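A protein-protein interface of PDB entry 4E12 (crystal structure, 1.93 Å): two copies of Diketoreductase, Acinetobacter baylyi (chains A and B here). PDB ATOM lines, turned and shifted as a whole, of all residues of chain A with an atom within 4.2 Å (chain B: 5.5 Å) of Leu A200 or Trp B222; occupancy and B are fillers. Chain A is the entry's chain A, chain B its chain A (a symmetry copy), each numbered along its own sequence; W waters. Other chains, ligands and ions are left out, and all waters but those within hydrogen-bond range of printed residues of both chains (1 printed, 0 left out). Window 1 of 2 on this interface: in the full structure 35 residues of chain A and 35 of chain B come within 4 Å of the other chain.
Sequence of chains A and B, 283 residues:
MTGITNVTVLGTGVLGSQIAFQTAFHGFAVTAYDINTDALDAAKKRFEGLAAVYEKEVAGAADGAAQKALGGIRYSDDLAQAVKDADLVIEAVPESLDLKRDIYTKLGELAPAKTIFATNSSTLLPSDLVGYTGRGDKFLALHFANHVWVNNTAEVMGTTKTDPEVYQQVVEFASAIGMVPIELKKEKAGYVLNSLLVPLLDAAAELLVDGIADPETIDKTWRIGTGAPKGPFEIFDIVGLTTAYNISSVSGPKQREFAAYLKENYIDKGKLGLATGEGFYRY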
ATOM      1  N   LEU A 196       4.380 -16.422 -31.382  1.00  0.00           N
ATOM      2  CA  LEU A 196       3.826 -15.714 -30.237  1.00  0.00           C
ATOM      3  C   LEU A 196       3.344 -16.671 -29.168  1.00  0.00           C
ATOM      4  O   LEU A 196       3.532 -16.425 -27.977  1.00  0.00           O
ATOM      5  CB  LEU A 196       2.647 -14.844 -30.666  1.00  0.00           C
ATOM      6  CG  LEU A 196       2.877 -13.694 -31.630  1.00  0.00           C
ATOM      7  CD1 LEU A 196       1.529 -13.041 -31.891  1.00  0.00           C
ATOM      8  CD2 LEU A 196       3.826 -12.699 -30.985  1.00  0.00           C
ATOM      9  N   LEU A 197       2.689 -17.752 -29.599  1.00  0.00           N
ATOM     10  CA  LEU A 197       2.069 -18.663 -28.662  1.00  0.00           C
ATOM     11  C   LEU A 197       3.056 -19.530 -27.896  1.00  0.00           C
ATOM     12  O   LEU A 197       2.879 -19.740 -26.697  1.00  0.00           O
ATOM     13  CB  LEU A 197       1.047 -19.543 -29.369  1.00  0.00           C
ATOM     14  CG  LEU A 197       0.260 -20.481 -28.475  1.00  0.00           C
ATOM     15  CD1 LEU A 197      -0.626 -19.696 -27.508  1.00  0.00           C
ATOM     16  CD2 LEU A 197      -0.564 -21.391 -29.361  1.00  0.00           C
ATOM     17  N   VAL A 198       4.084 -20.058 -28.554  1.00  0.00           N
ATOM     18  CA  VAL A 198       4.997 -20.951 -27.848  1.00  0.00           C
ATOM     19  C   VAL A 198       5.638 -20.275 -26.640  1.00  0.00           C
ATOM     20  O   VAL A 198       5.737 -20.890 -25.579  1.00  0.00           O
ATOM     21  CB  VAL A 198       6.050 -21.577 -28.795  1.00  0.00           C
ATOM     22  CG1 VAL A 198       7.158 -22.255 -27.986  1.00  0.00           C
ATOM     23  CG2 VAL A 198       5.350 -22.600 -29.686  1.00  0.00           C
ATOM     24  N   PRO A 199       6.088 -19.008 -26.773  1.00  0.00           N
ATOM     25  CA  PRO A 199       6.684 -18.387 -25.581  1.00  0.00           C
ATOM     26  C   PRO A 199       5.744 -18.250 -24.377  1.00  0.00           C
ATOM     27  O   PRO A 199       6.150 -18.412 -23.218  1.00  0.00           O
ATOM     28  CB  PRO A 199       7.205 -17.039 -26.105  1.00  0.00           C
ATOM     29  CG  PRO A 199       7.475 -17.296 -27.547  1.00  0.00           C
ATOM     30  CD  PRO A 199       6.369 -18.229 -27.996  1.00  0.00           C
ATOM     31  N   LEU A 200       4.474 -17.984 -24.653  1.00  0.00           N
ATOM     32  CA  LEU A 200       3.465 -17.932 -23.594  1.00  0.00           C
ATOM     33  C   LEU A 200       3.287 -19.313 -22.922  1.00  0.00           C
ATOM     34  O   LEU A 200       3.300 -19.437 -21.690  1.00  0.00           O
ATOM     35  CB  LEU A 200       2.132 -17.448 -24.183  1.00  0.00           C
ATOM     36  CG  LEU A 200       0.953 -17.420 -23.217  1.00  0.00           C
ATOM     37  CD1 LEU A 200       1.325 -16.538 -22.007  1.00  0.00           C
ATOM     38  CD2 LEU A 200      -0.293 -16.906 -23.960  1.00  0.00           C
ATOM     39  N   LEU A 201       3.153 -20.352 -23.738  1.00  0.00           N
ATOM     40  CA  LEU A 201       2.951 -21.695 -23.209  1.00  0.00           C
ATOM     41  C   LEU A 201       4.193 -22.220 -22.489  1.00  0.00           C
ATOM     42  O   LEU A 201       4.048 -22.906 -21.479  1.00  0.00           O
ATOM     43  CB  LEU A 201       2.507 -22.673 -24.296  1.00  0.00           C
ATOM     44  CG  LEU A 201       1.205 -22.323 -25.013  1.00  0.00           C
ATOM     45  CD1 LEU A 201       0.892 -23.382 -26.064  1.00  0.00           C
ATOM     46  CD2 LEU A 201       0.049 -22.203 -24.026  1.00  0.00           C
ATOM     47  N   ASP A 202       5.385 -21.923 -23.015  1.00  0.00           N
ATOM     48  CA  ASP A 202       6.637 -22.271 -22.324  1.00  0.00           C
ATOM     49  C   ASP A 202       6.727 -21.594 -20.968  1.00  0.00           C
ATOM     50  O   ASP A 202       7.214 -22.188 -20.001  1.00  0.00           O
ATOM     51  CB  ASP A 202       7.870 -21.865 -23.137  1.00  0.00           C
ATOM     52  CG  ASP A 202       8.091 -22.741 -24.346  1.00  0.00           C
ATOM     53  OD1 ASP A 202       7.375 -23.755 -24.496  1.00  0.00           O
ATOM     54  OD2 ASP A 202       8.989 -22.416 -25.144  1.00  0.00           O
ATOM     55  N   ALA A 203       6.291 -20.337 -20.897  1.00  0.00           N
ATOM     56  CA  ALA A 203       6.315 -19.617 -19.625  1.00  0.00           C
ATOM     57  C   ALA A 203       5.357 -20.247 -18.614  1.00  0.00           C
ATOM     58  O   ALA A 203       5.689 -20.392 -17.438  1.00  0.00           O
ATOM     59  CB  ALA A 203       5.946 -18.154 -19.832  1.00  0.00           C
ATOM     60  N   ALA A 204       4.153 -20.586 -19.044  1.00  0.00           N
ATOM     61  CA  ALA A 204       3.185 -21.209 -18.134  1.00  0.00           C
ATOM     62  C   ALA A 204       3.711 -22.567 -17.630  1.00  0.00           C
ATOM     63  O   ALA A 204       3.585 -22.917 -16.448  1.00  0.00           O
ATOM     64  CB  ALA A 204       1.847 -21.396 -18.854  1.00  0.00           C
ATOM     65  N   TRP A 222      -3.965 -15.170 -16.320  1.00  0.00           N
ATOM     66  CA  TRP A 222      -3.923 -14.727 -17.708  1.00  0.00           C
ATOM     67  C   TRP A 222      -5.247 -14.147 -18.169  1.00  0.00           C
ATOM     68  O   TRP A 222      -5.273 -13.120 -18.859  1.00  0.00           O
ATOM     69  CB  TRP A 222      -3.511 -15.864 -18.636  1.00  0.00           C
ATOM     70  CG  TRP A 222      -3.223 -15.422 -20.034  1.00  0.00           C
ATOM     71  CD1 TRP A 222      -3.931 -15.754 -21.155  1.00  0.00           C
ATOM     72  CD2 TRP A 222      -2.140 -14.580 -20.478  1.00  0.00           C
ATOM     73  NE1 TRP A 222      -3.349 -15.194 -22.264  1.00  0.00           N
ATOM     74  CE2 TRP A 222      -2.248 -14.471 -21.882  1.00  0.00           C
ATOM     75  CE3 TRP A 222      -1.088 -13.916 -19.825  1.00  0.00           C
ATOM     76  CZ2 TRP A 222      -1.333 -13.724 -22.654  1.00  0.00           C
ATOM     77  CZ3 TRP A 222      -0.195 -13.181 -20.580  1.00  0.00           C
ATOM     78  CH2 TRP A 222      -0.316 -13.089 -21.981  1.00  0.00           C
ATOM     79  N   LEU B 196       4.201 -14.423 -17.494  1.00  0.00           N
ATOM     80  CA  LEU B 196       3.515 -14.889 -18.689  1.00  0.00           C
ATOM     81  C   LEU B 196       3.513 -13.838 -19.778  1.00  0.00           C
ATOM     82  O   LEU B 196       3.688 -14.154 -20.954  1.00  0.00           O
ATOM     83  CB  LEU B 196       2.065 -15.245 -18.368  1.00  0.00           C
ATOM     84  CG  LEU B 196       1.770 -16.383 -17.406  1.00  0.00           C
ATOM     85  CD1 LEU B 196       0.260 -16.478 -17.262  1.00  0.00           C
ATOM     86  CD2 LEU B 196       2.324 -17.672 -17.990  1.00  0.00           C
ATOM     87  N   LEU B 197       3.279 -12.583 -19.384  1.00  0.00           N
ATOM     88  CA  LEU B 197       3.122 -11.521 -20.351  1.00  0.00           C
ATOM     89  C   LEU B 197       4.421 -11.099 -21.025  1.00  0.00           C
ATOM     90  O   LEU B 197       4.431 -10.857 -22.231  1.00  0.00           O
ATOM     91  CB  LEU B 197       2.453 -10.311 -19.714  1.00  0.00           C
ATOM     92  CG  LEU B 197       2.150  -9.160 -20.653  1.00  0.00           C
ATOM     93  CD1 LEU B 197       1.113  -9.569 -21.699  1.00  0.00           C
ATOM     94  CD2 LEU B 197       1.661  -7.993 -19.821  1.00  0.00           C
ATOM     95  N   PRO B 199       7.112 -12.738 -21.914  1.00  0.00           N
ATOM     96  CA  PRO B 199       7.524 -13.555 -23.064  1.00  0.00           C
ATOM     97  C   PRO B 199       6.699 -13.349 -24.340  1.00  0.00           C
ATOM     98  O   PRO B 199       7.226 -13.368 -25.461  1.00  0.00           O
ATOM     99  CB  PRO B 199       7.458 -14.992 -22.521  1.00  0.00           C
ATOM    100  CG  PRO B 199       7.690 -14.834 -21.059  1.00  0.00           C
ATOM    101  CD  PRO B 199       6.984 -13.547 -20.684  1.00  0.00           C
ATOM    102  N   LEU B 200       5.404 -13.115 -24.169  1.00  0.00           N
ATOM    103  CA  LEU B 200       4.537 -12.800 -25.305  1.00  0.00           C
ATOM    104  C   LEU B 200       4.943 -11.464 -25.967  1.00  0.00           C
ATOM    105  O   LEU B 200       5.099 -11.373 -27.193  1.00  0.00           O
ATOM    106  CB  LEU B 200       3.078 -12.738 -24.831  1.00  0.00           C
ATOM    107  CG  LEU B 200       2.054 -12.338 -25.886  1.00  0.00           C
ATOM    108  CD1 LEU B 200       2.162 -13.313 -27.077  1.00  0.00           C
ATOM    109  CD2 LEU B 200       0.652 -12.335 -25.251  1.00  0.00           C
ATOM    110  N   THR B 217      -0.609  -6.705 -38.200  1.00  0.00           N
ATOM    111  CA  THR B 217      -0.641  -8.097 -38.585  1.00  0.00           C
ATOM    112  C   THR B 217      -0.370  -9.009 -37.382  1.00  0.00           C
ATOM    113  O   THR B 217      -1.004 -10.055 -37.211  1.00  0.00           O
ATOM    114  CB  THR B 217       0.406  -8.352 -39.668  1.00  0.00           C
ATOM    115  OG1 THR B 217       0.079  -7.561 -40.805  1.00  0.00           O
ATOM    116  CG2 THR B 217       0.422  -9.801 -40.078  1.00  0.00           C
ATOM    117  N   ILE B 218       0.571  -8.609 -36.550  1.00  0.00           N
ATOM    118  CA  ILE B 218       0.932  -9.408 -35.378  1.00  0.00           C
ATOM    119  C   ILE B 218      -0.266  -9.450 -34.427  1.00  0.00           C
ATOM    120  O   ILE B 218      -0.646 -10.520 -33.929  1.00  0.00           O
ATOM    121  CB  ILE B 218       2.202  -8.818 -34.722  1.00  0.00           C
ATOM    122  CG1 ILE B 218       3.351  -8.856 -35.745  1.00  0.00           C
ATOM    123  CG2 ILE B 218       2.545  -9.545 -33.441  1.00  0.00           C
ATOM    124  CD1 ILE B 218       4.621  -8.172 -35.309  1.00  0.00           C
ATOM    125  N   ASP B 219      -0.886  -8.293 -34.202  1.00  0.00           N
ATOM    126  CA  ASP B 219      -2.035  -8.237 -33.311  1.00  0.00           C
ATOM    127  C   ASP B 219      -3.227  -9.044 -33.817  1.00  0.00           C
ATOM    128  O   ASP B 219      -3.825  -9.784 -33.033  1.00  0.00           O
ATOM    129  CB  ASP B 219      -2.463  -6.802 -33.009  1.00  0.00           C
ATOM    130  CG  ASP B 219      -1.521  -6.095 -32.045  1.00  0.00           C
ATOM    131  OD1 ASP B 219      -0.559  -6.726 -31.556  1.00  0.00           O
ATOM    132  OD2 ASP B 219      -1.754  -4.904 -31.758  1.00  0.00           O
ATOM    133  N   LYS B 220      -3.590  -8.911 -35.099  1.00  0.00           N
ATOM    134  CA  LYS B 220      -4.752  -9.659 -35.585  1.00  0.00           C
ATOM    135  C   LYS B 220      -4.486 -11.172 -35.509  1.00  0.00           C
ATOM    136  O   LYS B 220      -5.378 -11.970 -35.194  1.00  0.00           O
ATOM    137  CB  LYS B 220      -5.224  -9.206 -36.984  1.00  0.00           C
ATOM    138  CG  LYS B 220      -4.316  -9.520 -38.152  1.00  0.00           C
ATOM    139  CD  LYS B 220      -4.940  -9.008 -39.466  1.00  0.00           C
ATOM    140  CE  LYS B 220      -4.004  -9.218 -40.654  1.00  0.00           C
ATOM    141  NZ  LYS B 220      -4.572  -8.682 -41.916  1.00  0.00           N
ATOM    142  N   THR B 221      -3.241 -11.567 -35.744  1.00  0.00           N
ATOM    143  CA  THR B 221      -2.893 -12.966 -35.601  1.00  0.00           C
ATOM    144  C   THR B 221      -3.189 -13.453 -34.192  1.00  0.00           C
ATOM    145  O   THR B 221      -3.751 -14.534 -34.014  1.00  0.00           O
ATOM    146  CB  THR B 221      -1.417 -13.223 -35.896  1.00  0.00           C
ATOM    147  OG1 THR B 221      -1.111 -12.809 -37.232  1.00  0.00           O
ATOM    148  CG2 THR B 221      -1.114 -14.700 -35.737  1.00  0.00           C
ATOM    149  N   TRP B 222      -2.790 -12.683 -33.183  1.00  0.00           N
ATOM    150  CA  TRP B 222      -3.026 -13.087 -31.803  1.00  0.00           C
ATOM    151  C   TRP B 222      -4.502 -13.120 -31.456  1.00  0.00           C
ATOM    152  O   TRP B 222      -4.967 -14.052 -30.787  1.00  0.00           O
ATOM    153  CB  TRP B 222      -2.291 -12.174 -30.828  1.00  0.00           C
ATOM    154  CG  TRP B 222      -2.302 -12.670 -29.418  1.00  0.00           C
ATOM    155  CD1 TRP B 222      -2.919 -12.080 -28.352  1.00  0.00           C
ATOM    156  CD2 TRP B 222      -1.652 -13.850 -28.904  1.00  0.00           C
ATOM    157  NE1 TRP B 222      -2.679 -12.800 -27.209  1.00  0.00           N
ATOM    158  CE2 TRP B 222      -1.904 -13.889 -27.515  1.00  0.00           C
ATOM    159  CE3 TRP B 222      -0.879 -14.870 -29.482  1.00  0.00           C
ATOM    160  CZ2 TRP B 222      -1.400 -14.913 -26.684  1.00  0.00           C
ATOM    161  CZ3 TRP B 222      -0.390 -15.875 -28.671  1.00  0.00           C
ATOM    162  CH2 TRP B 222      -0.646 -15.893 -27.285  1.00  0.00           C
ATOM    163  N   ARG B 223      -5.242 -12.109 -31.908  1.00  0.00           N
ATOM    164  CA  ARG B 223      -6.658 -12.030 -31.589  1.00  0.00           C
ATOM    165  C   ARG B 223      -7.425 -13.184 -32.222  1.00  0.00           C
ATOM    166  O   ARG B 223      -8.240 -13.834 -31.562  1.00  0.00           O
ATOM    167  CB  ARG B 223      -7.241 -10.687 -32.000  1.00  0.00           C
ATOM    168  CG  ARG B 223      -6.648  -9.508 -31.239  1.00  0.00           C
ATOM    169  CD  ARG B 223      -7.519  -8.277 -31.409  1.00  0.00           C
ATOM    170  NE  ARG B 223      -7.794  -8.039 -32.816  1.00  0.00           N
ATOM    171  CZ  ARG B 223      -7.112  -7.217 -33.605  1.00  0.00           C
ATOM    172  NH1 ARG B 223      -6.080  -6.530 -33.128  1.00  0.00           N
ATOM    173  NH2 ARG B 223      -7.466  -7.075 -34.881  1.00  0.00           N
ATOM    174  N   ILE B 224      -7.135 -13.460 -33.485  1.00  0.00           N
ATOM    175  CA  ILE B 224      -7.802 -14.529 -34.209  1.00  0.00           C
ATOM    176  C   ILE B 224      -7.349 -15.899 -33.726  1.00  0.00           C
ATOM    177  O   ILE B 224      -8.163 -16.816 -33.572  1.00  0.00           O
ATOM    178  CB  ILE B 224      -7.553 -14.410 -35.724  1.00  0.00           C
ATOM    179  CG1 ILE B 224      -8.183 -13.112 -36.244  1.00  0.00           C
ATOM    180  CG2 ILE B 224      -8.081 -15.634 -36.460  1.00  0.00           C
ATOM    181  CD1 ILE B 224      -8.040 -12.905 -37.731  1.00  0.00           C
ATOM    182  N   GLY B 225      -6.050 -16.031 -33.483  1.00  0.00           N
ATOM    183  CA  GLY B 225      -5.493 -17.323 -33.134  1.00  0.00           C
ATOM    184  C   GLY B 225      -5.782 -17.790 -31.726  1.00  0.00           C
ATOM    185  O   GLY B 225      -5.816 -18.997 -31.470  1.00  0.00           O
ATOM    186  N   THR B 226      -6.007 -16.859 -30.805  1.00  0.00           N
ATOM    187  CA  THR B 226      -6.243 -17.255 -29.416  1.00  0.00           C
ATOM    188  C   THR B 226      -7.576 -16.728 -28.894  1.00  0.00           C
ATOM    189  O   THR B 226      -7.980 -17.063 -27.777  1.00  0.00           O
ATOM    190  CB  THR B 226      -5.134 -16.726 -28.476  1.00  0.00           C
ATOM    191  OG1 THR B 226      -5.182 -15.287 -28.444  1.00  0.00           O
ATOM    192  CG2 THR B 226      -3.769 -17.166 -28.982  1.00  0.00           C
ATOM    193  N   GLY B 227      -8.243 -15.884 -29.676  1.00  0.00           N
ATOM    194  CA  GLY B 227      -9.460 -15.273 -29.193  1.00  0.00           C
ATOM    195  C   GLY B 227      -9.252 -14.129 -28.226  1.00  0.00           C
ATOM    196  O   GLY B 227     -10.229 -13.547 -27.748  1.00  0.00           O
ATOM    197  N   ALA B 228      -7.998 -13.804 -27.916  1.00  0.00           N
ATOM    198  CA  ALA B 228      -7.704 -12.689 -27.016  1.00  0.00           C
ATOM    199  C   ALA B 228      -8.305 -11.410 -27.604  1.00  0.00           C
ATOM    200  O   ALA B 228      -8.355 -11.241 -28.825  1.00  0.00           O
ATOM    201  CB  ALA B 228      -6.201 -12.538 -26.806  1.00  0.00           C
ATOM    202  N   LYS B 230      -7.192  -8.248 -27.324  1.00  0.00           N
ATOM    203  CA  LYS B 230      -6.180  -7.276 -27.741  1.00  0.00           C
ATOM    204  C   LYS B 230      -4.870  -8.013 -28.023  1.00  0.00           C
ATOM    205  O   LYS B 230      -4.502  -8.942 -27.298  1.00  0.00           O
ATOM    206  CB  LYS B 230      -5.949  -6.229 -26.654  1.00  0.00           C
ATOM    207  CG  LYS B 230      -7.197  -5.380 -26.326  1.00  0.00           C
ATOM    208  CD  LYS B 230      -6.934  -4.438 -25.188  1.00  0.00           C
ATOM    209  CE  LYS B 230      -8.204  -3.667 -24.839  1.00  0.00           C
ATOM    210  NZ  LYS B 230      -8.728  -2.974 -26.047  1.00  0.00           N
ATOM    211  N   GLY B 231      -4.177  -7.604 -29.077  1.00  0.00           N
ATOM    212  CA  GLY B 231      -2.886  -8.199 -29.372  1.00  0.00           C
ATOM    213  C   GLY B 231      -1.730  -7.514 -28.655  1.00  0.00           C
ATOM    214  O   GLY B 231      -1.914  -6.475 -28.011  1.00  0.00           O
ATOM    215  N   PRO B 232      -0.509  -8.072 -28.749  1.00  0.00           N
ATOM    216  CA  PRO B 232       0.657  -7.489 -28.087  1.00  0.00           C
ATOM    217  C   PRO B 232       0.843  -5.988 -28.210  1.00  0.00           C
ATOM    218  O   PRO B 232       1.250  -5.332 -27.248  1.00  0.00           O
ATOM    219  CB  PRO B 232       1.834  -8.279 -28.674  1.00  0.00           C
ATOM    220  CG  PRO B 232       1.219  -9.601 -29.043  1.00  0.00           C
ATOM    221  CD  PRO B 232      -0.158  -9.259 -29.544  1.00  0.00           C
HETATM  222  O   HOH W   1      -4.469 -15.367 -25.142  1.00  0.00           O
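The backbone carbonyl oxygen of Trp B222 lies within hydrogen-bond range of the side-chain hydroxyl of Thr B226 (2.7 Å).
Water W1 lies within hydrogen-bond range of NE1 of Trp A222 (3.1 Å) and OG1 of Thr B226 (3.4 Å).
Among the printed residues, pairs that only touch across the chains: Trp A222 with Leu B200 (3.5 Å), Leu A200 with Trp B222 (3.5 Å), Leu A196 with Leu B200 (3.5 Å), Leu A200 with Leu B196 (3.5 Å), Ala A204 with Leu B196 (3.6 Å), Trp A222 with Leu B197 (3.7 Å), Leu A197 with Trp B222 (3.7 Å), Trp A222 with Leu B196 (3.7 Å), Leu A196 with Trp B222 (3.7 Å), Pro A199 with Pro B199 (3.7 Å), Leu A196 with Ile B218 (3.9 Å) and Ala A203 with Pro B199 (3.9 Å).
Of the printed residues of chain B, Leu A196 touches Leu B200 (3.5 Å), Ile B218 (3.9 Å) and Trp B222 (3.7 Å). Leu A200 touches two residues of chain B. Asp A202 touches none of the printed residues of chain B. Of the printed residues of chain B, Ala A204 touches Leu B196 (3.6 Å). Of the printed residues of chain B, Trp A222 touches Leu B196 (3.7 Å), Leu B197 (3.7 Å) and Leu B200 (3.5 Å). Of the printed residues of chain A, Pro B199 touches Pro A199 and Ala A203. Trp B222 touches three residues of chain A.
Hydrophobic or aromatic side chains of chain A within 4 Å of the printed part of chain B: Leu A196, Leu A197, Pro A199, Leu A200, Ala A203, Ala A204 and Trp A222. Of the 19 printed residues of chain B, 6 touch a printed residue of chain A. Printed residues of chain B that touch a printed residue of chain A: Leu B196, Leu B197, Pro B199, Leu B200, Ile B218 and Trp B222. Among the printed residues, 12 pairs touch across the chains. Among the printed residues, no Asp or Glu carboxylate lies within 4 Å of a Lys or Arg side-chain nitrogen of the other chain.
Leu A196 touches Leu B200, and with the chains exchanged Leu A200 touches Leu B196. Leu A197 touches Trp B222, and with the chains exchanged Trp A222 touches Leu B197. Pro B199 touches its own counterpart, Pro A199. Leu A200 touches Trp B222, and with the chains exchanged Trp A222 touches Leu B200. 5 positions are printed for both chains. Of the 12 pairs that touch across the chains among the printed residues, 9 have their exchanged pair printed and touching as well.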
